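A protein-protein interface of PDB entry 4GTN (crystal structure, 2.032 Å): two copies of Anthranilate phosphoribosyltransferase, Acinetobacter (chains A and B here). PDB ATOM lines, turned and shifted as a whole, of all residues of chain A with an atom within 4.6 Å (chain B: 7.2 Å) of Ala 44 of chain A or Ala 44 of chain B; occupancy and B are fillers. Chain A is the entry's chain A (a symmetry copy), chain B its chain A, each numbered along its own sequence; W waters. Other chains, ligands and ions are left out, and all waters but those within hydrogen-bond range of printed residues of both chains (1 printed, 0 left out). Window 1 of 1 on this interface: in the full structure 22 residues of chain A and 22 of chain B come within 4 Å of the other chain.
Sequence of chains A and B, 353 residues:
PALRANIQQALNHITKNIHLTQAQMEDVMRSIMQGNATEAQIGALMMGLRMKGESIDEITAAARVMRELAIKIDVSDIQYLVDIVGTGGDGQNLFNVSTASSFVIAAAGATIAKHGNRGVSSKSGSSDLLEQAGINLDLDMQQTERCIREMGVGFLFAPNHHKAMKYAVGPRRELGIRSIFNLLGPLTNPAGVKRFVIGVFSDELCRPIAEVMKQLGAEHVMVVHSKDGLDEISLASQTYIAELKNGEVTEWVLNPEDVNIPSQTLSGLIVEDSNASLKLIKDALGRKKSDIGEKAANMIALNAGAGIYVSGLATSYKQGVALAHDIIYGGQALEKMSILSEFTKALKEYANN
N of Thr 38 of chain B sits at hydrogen-bond distance from OE1 of Gln 41 of chain B (3.0 Å).
Ala 40 of chain A touches Ala 40 of chain B. CB of Ala 44 of chain B touches O of Gly 43 of chain A (3.6 Å). CB of Ala 44 of chain A touches O of Gly 43 of chain B (3.6 Å). Leu 175 of chain B touches Ala 44 of chain A. Met 47 of chain A touches Leu 11 of chain B (CE to O, 3.4 Å). CE of Met 47 of chain A touches CG2 of Ile 14 of chain B, 3.6 Å away. Gly 48 of chain B touches Met 47 of chain A. Met 47 of chain B touches Gly 48 of chain A. Leu 175 of chain A touches Leu 11 of chain B. Ala 40 of chain B touches Leu 175 of chain A.
Of the printed residues of chain B, Ala 44 of chain A touches Gly 43 (3.6 Å), Ala 44 (3.99 Å), Met 47 (3.3 Å) and Leu 175 (3.8 Å). Printed residues of chain A within 4 Å of Glu 39 of chain B: Ala 40 (3.5 Å). Of the printed residues of chain A, Ala 44 of chain B touches Gly 43 (3.6 Å), Ala 44 (3.99 Å), Met 47 (3.3 Å) and Leu 175 (3.8 Å). Of the printed residues of chain A, Met 47 of chain B touches Leu 11, Ala 44 and Gly 48. The nearest printed residue of chain B that does not touch Ala 44 of chain A is Ala 40 of chain B (4.6 Å). The nearest printed residue of chain A that does not touch Ala 44 of chain B is Ala 40 of chain A (4.6 Å). The nearest printed residue of chain A that does not touch Met 51 of chain B is Met 47 of chain A (5.2 Å).
Of the 11 printed residues of chain A, 8 touch a printed residue of chain B. Printed residues of chain A that touch a printed residue of chain B: Leu 11, Ala 40, Gln 41, Gly 43, Ala 44, Met 47, Gly 48 and Leu 175. Of the 18 printed residues of chain B, 11 touch a printed residue of chain A. Hydrophobic or aromatic side chains of chain B that line the printed part of chain A: Leu 11, Ile 14, Ala 44, Met 47, Met 51 and Leu 175.
Leu 11 of chain A touches Leu 175 of chain B, and with the chains exchanged Leu 175 of chain A touches Leu 11 of chain B. Ala 40 of chain A touches its own counterpart, Ala 40 of chain B. Ala 40 of chain A touches Gly 43 of chain B, and with the chains exchanged Gly 43 of chain A touches Ala 40 of chain B. Ala 44 of chain A touches Leu 175 of chain B, and with the chains exchanged Leu 175 of chain A touches Ala 44 of chain B. Of the 23 pairs that touch across the chains among the printed residues, 20 have their exchanged pair printed and touching as well.
Water W1 bridges OE1 of Glu 39 of chain B (2.5 Å) and N of Ala 40 of chain A (3.0 Å).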
ATOM      1  N   LEU A  11     -16.424  -4.131 -14.148  1.00  0.00           N
ATOM      2  CA  LEU A  11     -15.756  -2.866 -14.434  1.00  0.00           C
ATOM      3  C   LEU A  11     -14.276  -3.016 -14.180  1.00  0.00           C
ATOM      4  O   LEU A  11     -13.452  -2.533 -14.957  1.00  0.00           O
ATOM      5  CB  LEU A  11     -16.299  -1.734 -13.603  1.00  0.00           C
ATOM      6  CG  LEU A  11     -17.703  -1.268 -13.924  1.00  0.00           C
ATOM      7  CD1 LEU A  11     -18.111  -0.336 -12.833  1.00  0.00           C
ATOM      8  CD2 LEU A  11     -17.735  -0.569 -15.284  1.00  0.00           C
ATOM      9  N   ALA A  40     -24.474   5.748 -12.872  1.00  0.00           N
ATOM     10  CA  ALA A  40     -23.039   5.909 -12.961  1.00  0.00           C
ATOM     11  C   ALA A  40     -22.395   4.629 -13.492  1.00  0.00           C
ATOM     12  O   ALA A  40     -21.501   4.682 -14.357  1.00  0.00           O
ATOM     13  CB  ALA A  40     -22.469   6.309 -11.605  1.00  0.00           C
ATOM     14  N   GLN A  41     -22.879   3.488 -12.999  1.00  0.00           N
ATOM     15  CA  GLN A  41     -22.402   2.203 -13.434  1.00  0.00           C
ATOM     16  C   GLN A  41     -22.632   2.036 -14.917  1.00  0.00           C
ATOM     17  O   GLN A  41     -21.746   1.545 -15.611  1.00  0.00           O
ATOM     18  CB  GLN A  41     -23.067   1.071 -12.675  1.00  0.00           C
ATOM     19  CG  GLN A  41     -22.440   0.797 -11.333  1.00  0.00           C
ATOM     20  CD  GLN A  41     -23.252  -0.160 -10.497  1.00  0.00           C
ATOM     21  OE1 GLN A  41     -24.320  -0.606 -10.907  1.00  0.00           O
ATOM     22  NE2 GLN A  41     -22.738  -0.504  -9.329  1.00  0.00           N
ATOM     23  N   ILE A  42     -23.796   2.473 -15.401  1.00  0.00           N
ATOM     24  CA  ILE A  42     -24.137   2.294 -16.819  1.00  0.00           C
ATOM     25  C   ILE A  42     -23.232   3.188 -17.662  1.00  0.00           C
ATOM     26  O   ILE A  42     -22.720   2.773 -18.687  1.00  0.00           O
ATOM     27  CB  ILE A  42     -25.641   2.600 -17.111  1.00  0.00           C
ATOM     28  CG1 ILE A  42     -26.560   1.575 -16.448  1.00  0.00           C
ATOM     29  CG2 ILE A  42     -25.908   2.559 -18.589  1.00  0.00           C
ATOM     30  CD1 ILE A  42     -28.053   1.931 -16.568  1.00  0.00           C
ATOM     31  N   GLY A  43     -23.018   4.420 -17.214  1.00  0.00           N
ATOM     32  CA  GLY A  43     -22.093   5.310 -17.900  1.00  0.00           C
ATOM     33  C   GLY A  43     -20.684   4.732 -17.972  1.00  0.00           C
ATOM     34  O   GLY A  43     -19.996   4.810 -18.996  1.00  0.00           O
ATOM     35  N   ALA A  44     -20.265   4.120 -16.877  1.00  0.00           N
ATOM     36  CA  ALA A  44     -18.936   3.552 -16.781  1.00  0.00           C
ATOM     37  C   ALA A  44     -18.768   2.339 -17.684  1.00  0.00           C
ATOM     38  O   ALA A  44     -17.714   2.175 -18.293  1.00  0.00           O
ATOM     39  CB  ALA A  44     -18.640   3.155 -15.336  1.00  0.00           C
ATOM     40  N   LEU A  45     -19.765   1.450 -17.678  1.00  0.00           N
ATOM     41  CA  LEU A  45     -19.786   0.252 -18.540  1.00  0.00           C
ATOM     42  C   LEU A  45     -19.737   0.627 -20.009  1.00  0.00           C
ATOM     43  O   LEU A  45     -18.920   0.113 -20.769  1.00  0.00           O
ATOM     44  CB  LEU A  45     -21.034  -0.581 -18.276  1.00  0.00           C
ATOM     45  CG  LEU A  45     -20.969  -1.410 -16.997  1.00  0.00           C
ATOM     46  CD1 LEU A  45     -22.333  -1.929 -16.584  1.00  0.00           C
ATOM     47  CD2 LEU A  45     -19.991  -2.570 -17.208  1.00  0.00           C
ATOM     48  N   MET A  46     -20.547   1.598 -20.381  1.00  0.00           N
ATOM     49  CA  MET A  46     -20.520   2.118 -21.742  1.00  0.00           C
ATOM     50  C   MET A  46     -19.162   2.675 -22.168  1.00  0.00           C
ATOM     51  O   MET A  46     -18.646   2.378 -23.277  1.00  0.00           O
ATOM     52  CB  MET A  46     -21.546   3.222 -21.868  1.00  0.00           C
ATOM     53  CG  MET A  46     -23.021   2.737 -21.855  1.00  0.00           C
ATOM     54  SD  MET A  46     -24.120   4.148 -21.802  1.00  0.00           S
ATOM     55  CE  MET A  46     -23.823   5.037 -23.318  1.00  0.00           C
ATOM     56  N   MET A  47     -18.591   3.515 -21.304  1.00  0.00           N
ATOM     57  CA  MET A  47     -17.317   4.097 -21.601  1.00  0.00           C
ATOM     58  C   MET A  47     -16.247   3.022 -21.558  1.00  0.00           C
ATOM     59  O   MET A  47     -15.368   3.012 -22.396  1.00  0.00           O
ATOM     60  CB  MET A  47     -16.975   5.205 -20.601  1.00  0.00           C
ATOM     61  CG  MET A  47     -15.848   6.102 -21.064  1.00  0.00           C
ATOM     62  SD  MET A  47     -16.316   7.266 -22.364  1.00  0.00           S
ATOM     63  CE  MET A  47     -14.774   8.190 -22.417  1.00  0.00           C
ATOM     64  N   GLY A  48     -16.303   2.123 -20.584  1.00  0.00           N
ATOM     65  CA  GLY A  48     -15.236   1.145 -20.451  1.00  0.00           C
ATOM     66  C   GLY A  48     -15.191   0.170 -21.630  1.00  0.00           C
ATOM     67  O   GLY A  48     -14.161  -0.102 -22.202  1.00  0.00           O
ATOM     68  N   LEU A 175     -24.107  10.877 -22.170  1.00  0.00           N
ATOM     69  CA  LEU A 175     -22.728  10.648 -22.616  1.00  0.00           C
ATOM     70  C   LEU A 175     -22.483  11.206 -24.001  1.00  0.00           C
ATOM     71  O   LEU A 175     -21.430  11.775 -24.293  1.00  0.00           O
ATOM     72  CB  LEU A 175     -22.350   9.172 -22.587  1.00  0.00           C
ATOM     73  CG  LEU A 175     -21.726   8.643 -21.300  1.00  0.00           C
ATOM     74  CD1 LEU A 175     -22.603   8.934 -20.113  1.00  0.00           C
ATOM     75  CD2 LEU A 175     -21.492   7.160 -21.397  1.00  0.00           C
ATOM     76  N   LEU B  11     -15.698  13.691 -23.179  1.00  0.00           N
ATOM     77  CA  LEU B  11     -15.808  12.237 -23.221  1.00  0.00           C
ATOM     78  C   LEU B  11     -15.398  11.746 -24.588  1.00  0.00           C
ATOM     79  O   LEU B  11     -14.693  10.744 -24.712  1.00  0.00           O
ATOM     80  CB  LEU B  11     -17.202  11.762 -22.911  1.00  0.00           C
ATOM     81  CG  LEU B  11     -17.678  11.933 -21.484  1.00  0.00           C
ATOM     82  CD1 LEU B  11     -19.139  11.636 -21.474  1.00  0.00           C
ATOM     83  CD2 LEU B  11     -16.918  10.987 -20.553  1.00  0.00           C
ATOM     84  N   ILE B  14     -11.692  11.765 -24.800  1.00  0.00           N
ATOM     85  CA  ILE B  14     -11.164  10.667 -24.025  1.00  0.00           C
ATOM     86  C   ILE B  14     -11.294   9.352 -24.785  1.00  0.00           C
ATOM     87  O   ILE B  14     -10.341   8.559 -24.787  1.00  0.00           O
ATOM     88  CB  ILE B  14     -11.819  10.595 -22.645  1.00  0.00           C
ATOM     89  CG1 ILE B  14     -11.408  11.824 -21.852  1.00  0.00           C
ATOM     90  CG2 ILE B  14     -11.416   9.326 -21.954  1.00  0.00           C
ATOM     91  CD1 ILE B  14     -12.242  12.071 -20.659  1.00  0.00           C
ATOM     92  N   THR B  38     -24.058  14.887 -14.794  1.00  0.00           N
ATOM     93  CA  THR B  38     -24.971  13.810 -14.389  1.00  0.00           C
ATOM     94  C   THR B  38     -24.165  12.669 -13.801  1.00  0.00           C
ATOM     95  O   THR B  38     -22.956  12.620 -13.972  1.00  0.00           O
ATOM     96  CB  THR B  38     -25.804  13.236 -15.585  1.00  0.00           C
ATOM     97  OG1 THR B  38     -24.958  12.451 -16.431  1.00  0.00           O
ATOM     98  CG2 THR B  38     -26.414  14.350 -16.399  1.00  0.00           C
ATOM     99  N   GLU B  39     -24.831  11.766 -13.099  1.00  0.00           N
ATOM    100  CA  GLU B  39     -24.173  10.614 -12.523  1.00  0.00           C
ATOM    101  C   GLU B  39     -23.536   9.717 -13.595  1.00  0.00           C
ATOM    102  O   GLU B  39     -22.392   9.277 -13.466  1.00  0.00           O
ATOM    103  CB  GLU B  39     -25.160   9.811 -11.685  1.00  0.00           C
ATOM    104  CG  GLU B  39     -25.501  10.449 -10.330  1.00  0.00           C
ATOM    105  CD  GLU B  39     -26.019   9.424  -9.320  1.00  0.00           C
ATOM    106  OE1 GLU B  39     -26.869   8.585  -9.696  1.00  0.00           O
ATOM    107  OE2 GLU B  39     -25.552   9.433  -8.152  1.00  0.00           O
ATOM    108  N   ALA B  40     -24.274   9.451 -14.664  1.00  0.00           N
ATOM    109  CA  ALA B  40     -23.749   8.625 -15.730  1.00  0.00           C
ATOM    110  C   ALA B  40     -22.490   9.260 -16.319  1.00  0.00           C
ATOM    111  O   ALA B  40     -21.488   8.564 -16.570  1.00  0.00           O
ATOM    112  CB  ALA B  40     -24.816   8.394 -16.792  1.00  0.00           C
ATOM    113  N   GLN B  41     -22.536  10.580 -16.500  1.00  0.00           N
ATOM    114  CA  GLN B  41     -21.413  11.323 -17.007  1.00  0.00           C
ATOM    115  C   GLN B  41     -20.225  11.165 -16.088  1.00  0.00           C
ATOM    116  O   GLN B  41     -19.113  10.978 -16.571  1.00  0.00           O
ATOM    117  CB  GLN B  41     -21.744  12.793 -17.180  1.00  0.00           C
ATOM    118  CG  GLN B  41     -22.467  13.099 -18.465  1.00  0.00           C
ATOM    119  CD  GLN B  41     -22.996  14.511 -18.511  1.00  0.00           C
ATOM    120  OE1 GLN B  41     -22.852  15.270 -17.558  1.00  0.00           O
ATOM    121  NE2 GLN B  41     -23.588  14.882 -19.634  1.00  0.00           N
ATOM    122  N   ILE B  42     -20.467  11.205 -14.776  1.00  0.00           N
ATOM    123  CA  ILE B  42     -19.367  11.126 -13.805  1.00  0.00           C
ATOM    124  C   ILE B  42     -18.769   9.722 -13.847  1.00  0.00           C
ATOM    125  O   ILE B  42     -17.562   9.555 -13.834  1.00  0.00           O
ATOM    126  CB  ILE B  42     -19.827  11.487 -12.357  1.00  0.00           C
ATOM    127  CG1 ILE B  42     -20.224  12.958 -12.245  1.00  0.00           C
ATOM    128  CG2 ILE B  42     -18.716  11.241 -11.376  1.00  0.00           C
ATOM    129  CD1 ILE B  42     -20.842  13.318 -10.881  1.00  0.00           C
ATOM    130  N   GLY B  43     -19.623   8.708 -13.919  1.00  0.00           N
ATOM    131  CA  GLY B  43     -19.143   7.341 -14.059  1.00  0.00           C
ATOM    132  C   GLY B  43     -18.297   7.155 -15.315  1.00  0.00           C
ATOM    133  O   GLY B  43     -17.256   6.489 -15.310  1.00  0.00           O
ATOM    134  N   ALA B  44     -18.742   7.775 -16.396  1.00  0.00           N
ATOM    135  CA  ALA B  44     -18.066   7.663 -17.672  1.00  0.00           C
ATOM    136  C   ALA B  44     -16.714   8.361 -17.664  1.00  0.00           C
ATOM    137  O   ALA B  44     -15.759   7.843 -18.238  1.00  0.00           O
ATOM    138  CB  ALA B  44     -18.938   8.255 -18.779  1.00  0.00           C
ATOM    139  N   LEU B  45     -16.674   9.574 -17.106  1.00  0.00           N
ATOM    140  CA  LEU B  45     -15.431  10.358 -16.965  1.00  0.00           C
ATOM    141  C   LEU B  45     -14.403   9.618 -16.130  1.00  0.00           C
ATOM    142  O   LEU B  45     -13.252   9.464 -16.529  1.00  0.00           O
ATOM    143  CB  LEU B  45     -15.716  11.711 -16.326  1.00  0.00           C
ATOM    144  CG  LEU B  45     -16.338  12.729 -17.276  1.00  0.00           C
ATOM    145  CD1 LEU B  45     -16.933  13.912 -16.536  1.00  0.00           C
ATOM    146  CD2 LEU B  45     -15.270  13.195 -18.271  1.00  0.00           C
ATOM    147  N   MET B  46     -14.852   9.074 -15.016  1.00  0.00           N
ATOM    148  CA  MET B  46     -13.987   8.251 -14.180  1.00  0.00           C
ATOM    149  C   MET B  46     -13.403   7.035 -14.898  1.00  0.00           C
ATOM    150  O   MET B  46     -12.182   6.743 -14.812  1.00  0.00           O
ATOM    151  CB  MET B  46     -14.776   7.763 -12.986  1.00  0.00           C
ATOM    152  CG  MET B  46     -15.104   8.859 -11.937  1.00  0.00           C
ATOM    153  SD  MET B  46     -16.206   8.195 -10.693  1.00  0.00           S
ATOM    154  CE  MET B  46     -15.288   6.894  -9.894  1.00  0.00           C
ATOM    155  N   MET B  47     -14.278   6.299 -15.583  1.00  0.00           N
ATOM    156  CA  MET B  47     -13.840   5.136 -16.294  1.00  0.00           C
ATOM    157  C   MET B  47     -12.982   5.557 -17.473  1.00  0.00           C
ATOM    158  O   MET B  47     -11.978   4.928 -17.743  1.00  0.00           O
ATOM    159  CB  MET B  47     -15.034   4.316 -16.793  1.00  0.00           C
ATOM    160  CG  MET B  47     -14.662   2.912 -17.212  1.00  0.00           C
ATOM    161  SD  MET B  47     -14.327   1.792 -15.834  1.00  0.00           S
ATOM    162  CE  MET B  47     -14.145   0.284 -16.796  1.00  0.00           C
ATOM    163  N   GLY B  48     -13.370   6.607 -18.185  1.00  0.00           N
ATOM    164  CA  GLY B  48     -12.631   6.972 -19.382  1.00  0.00           C
ATOM    165  C   GLY B  48     -11.212   7.450 -19.065  1.00  0.00           C
ATOM    166  O   GLY B  48     -10.245   7.045 -19.668  1.00  0.00           O
ATOM    167  N   LEU B  49     -11.099   8.332 -18.094  1.00  0.00           N
ATOM    168  CA  LEU B  49      -9.783   8.834 -17.662  1.00  0.00           C
ATOM    169  C   LEU B  49      -8.934   7.698 -17.123  1.00  0.00           C
ATOM    170  O   LEU B  49      -7.735   7.667 -17.376  1.00  0.00           O
ATOM    171  CB  LEU B  49      -9.958   9.881 -16.571  1.00  0.00           C
ATOM    172  CG  LEU B  49     -10.635  11.178 -17.011  1.00  0.00           C
ATOM    173  CD1 LEU B  49     -11.101  11.969 -15.782  1.00  0.00           C
ATOM    174  CD2 LEU B  49      -9.714  12.023 -17.873  1.00  0.00           C
ATOM    175  N   ARG B  50      -9.557   6.752 -16.410  1.00  0.00           N
ATOM    176  CA  ARG B  50      -8.820   5.618 -15.820  1.00  0.00           C
ATOM    177  C   ARG B  50      -8.205   4.776 -16.938  1.00  0.00           C
ATOM    178  O   ARG B  50      -7.049   4.377 -16.882  1.00  0.00           O
ATOM    179  CB  ARG B  50      -9.744   4.777 -14.928  1.00  0.00           C
ATOM    180  CG  ARG B  50      -9.261   3.380 -14.532  1.00  0.00           C
ATOM    181  CD  ARG B  50      -8.063   3.376 -13.625  1.00  0.00           C
ATOM    182  NE  ARG B  50      -7.522   2.029 -13.433  1.00  0.00           N
ATOM    183  CZ  ARG B  50      -7.898   1.148 -12.511  1.00  0.00           C
ATOM    184  NH1 ARG B  50      -8.859   1.412 -11.633  1.00  0.00           N
ATOM    185  NH2 ARG B  50      -7.303  -0.046 -12.483  1.00  0.00           N
ATOM    186  N   MET B  51      -8.966   4.535 -17.990  1.00  0.00           N
ATOM    187  CA  MET B  51      -8.463   3.644 -19.030  1.00  0.00           C
ATOM    188  C   MET B  51      -7.523   4.315 -20.015  1.00  0.00           C
ATOM    189  O   MET B  51      -6.575   3.714 -20.474  1.00  0.00           O
ATOM    190  CB  MET B  51      -9.620   2.988 -19.712  1.00  0.00           C
ATOM    191  CG  MET B  51     -10.060   1.837 -18.865  1.00  0.00           C
ATOM    192  SD  MET B  51     -11.458   1.122 -19.574  1.00  0.00           S
ATOM    193  CE  MET B  51     -10.707   0.092 -20.845  1.00  0.00           C
ATOM    194  N   LEU B 175     -19.027   2.418  -8.672  1.00  0.00           N
ATOM    195  CA  LEU B 175     -18.054   1.849  -9.611  1.00  0.00           C
ATOM    196  C   LEU B 175     -17.107   0.887  -8.928  1.00  0.00           C
ATOM    197  O   LEU B 175     -16.748  -0.161  -9.468  1.00  0.00           O
ATOM    198  CB  LEU B 175     -17.253   2.925 -10.334  1.00  0.00           C
ATOM    199  CG  LEU B 175     -17.815   3.434 -11.658  1.00  0.00           C
ATOM    200  CD1 LEU B 175     -19.229   3.919 -11.496  1.00  0.00           C
ATOM    201  CD2 LEU B 175     -16.962   4.547 -12.201  1.00  0.00           C
ATOM    202  N   ILE B 177     -14.050   1.198  -8.561  1.00  0.00           N
ATOM    203  CA  ILE B 177     -12.694   1.191  -9.123  1.00  0.00           C
ATOM    204  C   ILE B 177     -11.867   2.317  -8.487  1.00  0.00           C
ATOM    205  O   ILE B 177     -12.420   3.318  -8.071  1.00  0.00           O
ATOM    206  CB  ILE B 177     -12.677   1.396 -10.675  1.00  0.00           C
ATOM    207  CG1 ILE B 177     -13.289   2.743 -11.058  1.00  0.00           C
ATOM    208  CG2 ILE B 177     -13.410   0.277 -11.393  1.00  0.00           C
ATOM    209  CD1 ILE B 177     -12.987   3.195 -12.517  1.00  0.00           C
HETATM  210  O   HOH W   1     -25.585   6.472 -10.164  1.00  0.00           O
